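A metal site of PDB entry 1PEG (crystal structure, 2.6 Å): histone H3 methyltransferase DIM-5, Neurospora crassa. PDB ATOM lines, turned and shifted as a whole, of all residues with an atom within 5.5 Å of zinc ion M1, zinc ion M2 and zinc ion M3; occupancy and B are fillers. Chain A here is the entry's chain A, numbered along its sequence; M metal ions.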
ATOM      1  N   GLY A  49       6.362  11.620  -6.063  1.00  0.00           N
ATOM      2  CA  GLY A  49       7.081  12.507  -6.936  1.00  0.00           C
ATOM      3  C   GLY A  49       8.148  13.093  -6.062  1.00  0.00           C
ATOM      4  O   GLY A  49       8.441  12.563  -4.998  1.00  0.00           O
ATOM      5  N   CYS A  50       8.741  14.203  -6.492  1.00  0.00           N
ATOM      6  CA  CYS A  50       9.763  14.874  -5.695  1.00  0.00           C
ATOM      7  C   CYS A  50       9.309  16.240  -5.147  1.00  0.00           C
ATOM      8  O   CYS A  50       8.696  17.046  -5.843  1.00  0.00           O
ATOM      9  CB  CYS A  50      11.086  14.987  -6.485  1.00  0.00           C
ATOM     10  SG  CYS A  50      11.077  16.016  -7.985  1.00  0.00           S
ATOM     11  N   CYS A  52      11.195  18.538  -4.231  1.00  0.00           N
ATOM     12  CA  CYS A  52      12.138  19.543  -4.659  1.00  0.00           C
ATOM     13  C   CYS A  52      11.412  20.878  -4.707  1.00  0.00           C
ATOM     14  O   CYS A  52      10.223  20.957  -5.020  1.00  0.00           O
ATOM     15  CB  CYS A  52      12.667  19.225  -6.069  1.00  0.00           C
ATOM     16  SG  CYS A  52      13.946  17.937  -6.164  1.00  0.00           S
ATOM     17  N   GLU A  57      15.541  21.684  -9.111  1.00  0.00           N
ATOM     18  CA  GLU A  57      16.926  21.336  -8.911  1.00  0.00           C
ATOM     19  C   GLU A  57      16.891  19.863  -8.830  1.00  0.00           C
ATOM     20  O   GLU A  57      17.327  19.219  -7.884  1.00  0.00           O
ATOM     21  CB  GLU A  57      17.517  21.959  -7.649  1.00  0.00           C
ATOM     22  N   CYS A  58      16.346  19.328  -9.937  1.00  0.00           N
ATOM     23  CA  CYS A  58      16.127  17.909 -10.075  1.00  0.00           C
ATOM     24  C   CYS A  58      17.233  17.319 -10.930  1.00  0.00           C
ATOM     25  O   CYS A  58      17.014  16.335 -11.636  1.00  0.00           O
ATOM     26  CB  CYS A  58      14.757  17.624 -10.735  1.00  0.00           C
ATOM     27  SG  CYS A  58      13.261  18.193  -9.849  1.00  0.00           S
ATOM     28  N   CYS A  63      17.276  14.655  -5.200  1.00  0.00           N
ATOM     29  CA  CYS A  63      15.915  14.344  -5.712  1.00  0.00           C
ATOM     30  C   CYS A  63      15.664  12.829  -5.664  1.00  0.00           C
ATOM     31  O   CYS A  63      16.473  12.038  -6.159  1.00  0.00           O
ATOM     32  CB  CYS A  63      15.801  14.895  -7.151  1.00  0.00           C
ATOM     33  SG  CYS A  63      14.221  14.678  -8.051  1.00  0.00           S
ATOM     34  N   GLN A  64      14.541  12.431  -5.064  1.00  0.00           N
ATOM     35  CA  GLN A  64      14.181  11.016  -4.921  1.00  0.00           C
ATOM     36  C   GLN A  64      13.811  10.320  -6.227  1.00  0.00           C
ATOM     37  O   GLN A  64      13.596   9.110  -6.244  1.00  0.00           O
ATOM     38  CB  GLN A  64      13.022  10.866  -3.924  1.00  0.00           C
ATOM     39  N   CYS A  65      13.743  11.085  -7.313  1.00  0.00           N
ATOM     40  CA  CYS A  65      13.397  10.546  -8.631  1.00  0.00           C
ATOM     41  C   CYS A  65      14.554   9.737  -9.220  1.00  0.00           C
ATOM     42  O   CYS A  65      14.351   8.837 -10.037  1.00  0.00           O
ATOM     43  CB  CYS A  65      12.996  11.711  -9.554  1.00  0.00           C
ATOM     44  SG  CYS A  65      11.372  12.425  -9.118  1.00  0.00           S
ATOM     45  N   GLU A 111      12.840  10.112 -15.112  1.00  0.00           N
ATOM     46  CA  GLU A 111      12.341  11.467 -15.320  1.00  0.00           C
ATOM     47  C   GLU A 111      11.306  11.839 -14.278  1.00  0.00           C
ATOM     48  O   GLU A 111      10.762  10.977 -13.590  1.00  0.00           O
ATOM     49  CB  GLU A 111      11.720  11.564 -16.700  1.00  0.00           C
ATOM     50  CG  GLU A 111      12.353  12.559 -17.634  1.00  0.00           C
ATOM     51  CD  GLU A 111      11.581  12.653 -18.939  1.00  0.00           C
ATOM     52  OE1 GLU A 111      11.301  13.770 -19.419  1.00  0.00           O
ATOM     53  OE2 GLU A 111      11.240  11.591 -19.469  1.00  0.00           O
ATOM     54  N   CYS A 112      11.043  13.144 -14.167  1.00  0.00           N
ATOM     55  CA  CYS A 112      10.057  13.647 -13.229  1.00  0.00           C
ATOM     56  C   CYS A 112       8.658  13.499 -13.859  1.00  0.00           C
ATOM     57  O   CYS A 112       8.548  13.000 -14.982  1.00  0.00           O
ATOM     58  CB  CYS A 112      10.353  15.115 -12.891  1.00  0.00           C
ATOM     59  SG  CYS A 112      11.537  15.330 -11.519  1.00  0.00           S
ATOM     60  N   HIS A 113       7.616  13.911 -13.143  1.00  0.00           N
ATOM     61  CA  HIS A 113       6.237  13.787 -13.627  1.00  0.00           C
ATOM     62  C   HIS A 113       5.250  14.706 -12.890  1.00  0.00           C
ATOM     63  O   HIS A 113       5.640  15.746 -12.368  1.00  0.00           O
ATOM     64  CB  HIS A 113       5.770  12.345 -13.476  1.00  0.00           C
ATOM     65  CG  HIS A 113       6.170  11.738 -12.183  1.00  0.00           C
ATOM     66  ND1 HIS A 113       7.152  10.778 -12.070  1.00  0.00           N
ATOM     67  CD2 HIS A 113       5.760  11.992 -10.916  1.00  0.00           C
ATOM     68  CE1 HIS A 113       7.324  10.464 -10.805  1.00  0.00           C
ATOM     69  NE2 HIS A 113       6.488  11.186 -10.081  1.00  0.00           N
ATOM     70  N   CYS A 116       5.744  15.664  -8.760  1.00  0.00           N
ATOM     71  CA  CYS A 116       6.830  16.388  -8.143  1.00  0.00           C
ATOM     72  C   CYS A 116       6.586  17.885  -8.007  1.00  0.00           C
ATOM     73  O   CYS A 116       5.833  18.479  -8.785  1.00  0.00           O
ATOM     74  CB  CYS A 116       8.097  16.146  -8.947  1.00  0.00           C
ATOM     75  SG  CYS A 116       8.172  14.497  -9.678  1.00  0.00           S
ATOM     76  N   CYS A 118       8.002  20.344  -8.968  1.00  0.00           N
ATOM     77  CA  CYS A 118       8.786  21.003  -9.999  1.00  0.00           C
ATOM     78  C   CYS A 118       7.874  21.163 -11.218  1.00  0.00           C
ATOM     79  O   CYS A 118       6.887  20.430 -11.357  1.00  0.00           O
ATOM     80  CB  CYS A 118      10.025  20.167 -10.333  1.00  0.00           C
ATOM     81  SG  CYS A 118       9.678  18.603 -11.185  1.00  0.00           S
ATOM     82  N   CYS A 122      11.312  21.556 -15.670  1.00  0.00           N
ATOM     83  CA  CYS A 122      12.185  20.711 -14.876  1.00  0.00           C
ATOM     84  C   CYS A 122      13.110  19.965 -15.839  1.00  0.00           C
ATOM     85  O   CYS A 122      12.682  19.118 -16.632  1.00  0.00           O
ATOM     86  CB  CYS A 122      11.418  19.688 -14.038  1.00  0.00           C
ATOM     87  SG  CYS A 122      12.518  18.365 -13.405  1.00  0.00           S
ATOM     88  N   ASN A 124      14.725  17.522 -15.917  1.00  0.00           N
ATOM     89  CA  ASN A 124      14.639  16.069 -15.988  1.00  0.00           C
ATOM     90  C   ASN A 124      13.256  15.622 -16.366  1.00  0.00           C
ATOM     91  O   ASN A 124      12.759  14.637 -15.848  1.00  0.00           O
ATOM     92  CB  ASN A 124      15.001  15.479 -14.642  1.00  0.00           C
ATOM     93  CG  ASN A 124      15.288  13.999 -14.712  1.00  0.00           C
ATOM     94  OD1 ASN A 124      15.314  13.429 -15.790  1.00  0.00           O
ATOM     95  ND2 ASN A 124      15.511  13.376 -13.559  1.00  0.00           N
HETATM   96 ZN    ZN M   1      11.733  17.617 -11.383  1.00  0.00          ZN
HETATM   97 ZN    ZN M   2      10.468  14.475  -9.573  1.00  0.00          ZN
HETATM   98 ZN    ZN M   3      13.237  16.758  -8.061  1.00  0.00          ZN
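The backbone NH (N) of Cys 65 sits close to the side-chain sulfur (SG) of Cys 63 (3.7 Å).
The side-chain sulfur (SG) of Cys 122 sits close to the backbone NH (N) of Asn 124 (3.4 Å).
The backbone NH (N) of Cys 112 is in hydrogen-bond range of the backbone carbonyl oxygen (O) of Asn 124 (2.8 Å).
The side-chain sulfur (SG) of Cys 116 lies close to the backbone NH (N) of His 113 (3.6 Å).
Five residues have an atom within 4 Å of zinc ion M1: Cys 50, Cys 58, Cys 112, Cys 118 and Cys 122.
The nearest printed residue that does not touch zinc ion M1 is Cys 116 (4.6 Å).
Four residues have an atom within 4 Å of zinc ion M2: Cys 50, Cys 65, Cys 112 and Cys 116.
Along chain A the residues within 4 Å of zinc ion M2 span positions 50 to 116.
The nearest printed residue that does not touch zinc ion M2 is Cys 63 (4.1 Å).
Of the 15 residues printed, 4 come within 4 Å of zinc ion M3.
The nearest printed residue that does not touch zinc ion M3 is Cys 112 (4.1 Å).
Zinc ion M1 is bound by the side-chain sulfur (SG) of Cys 58 (2.2 Å), the side-chain sulfur (SG) of Cys 118 (2.3 Å), the side-chain sulfur (SG) of Cys 122 (2.3 Å) and the side-chain sulfur (SG) of Cys 112 (2.3 Å).
Zinc ion M1 has four donor atoms within binding distance.
Zinc ion M2 is bound by SG of Cys 65, SG of Cys 50, SG of Cys 116 and SG of Cys 112.
Zinc ion M2 has four donor atoms within binding distance.
Zinc ion M3 is bound by SG of Cys 50 (2.3 Å), SG of Cys 58 (2.3 Å), SG of Cys 63 (2.3 Å) and SG of Cys 52 (2.3 Å).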
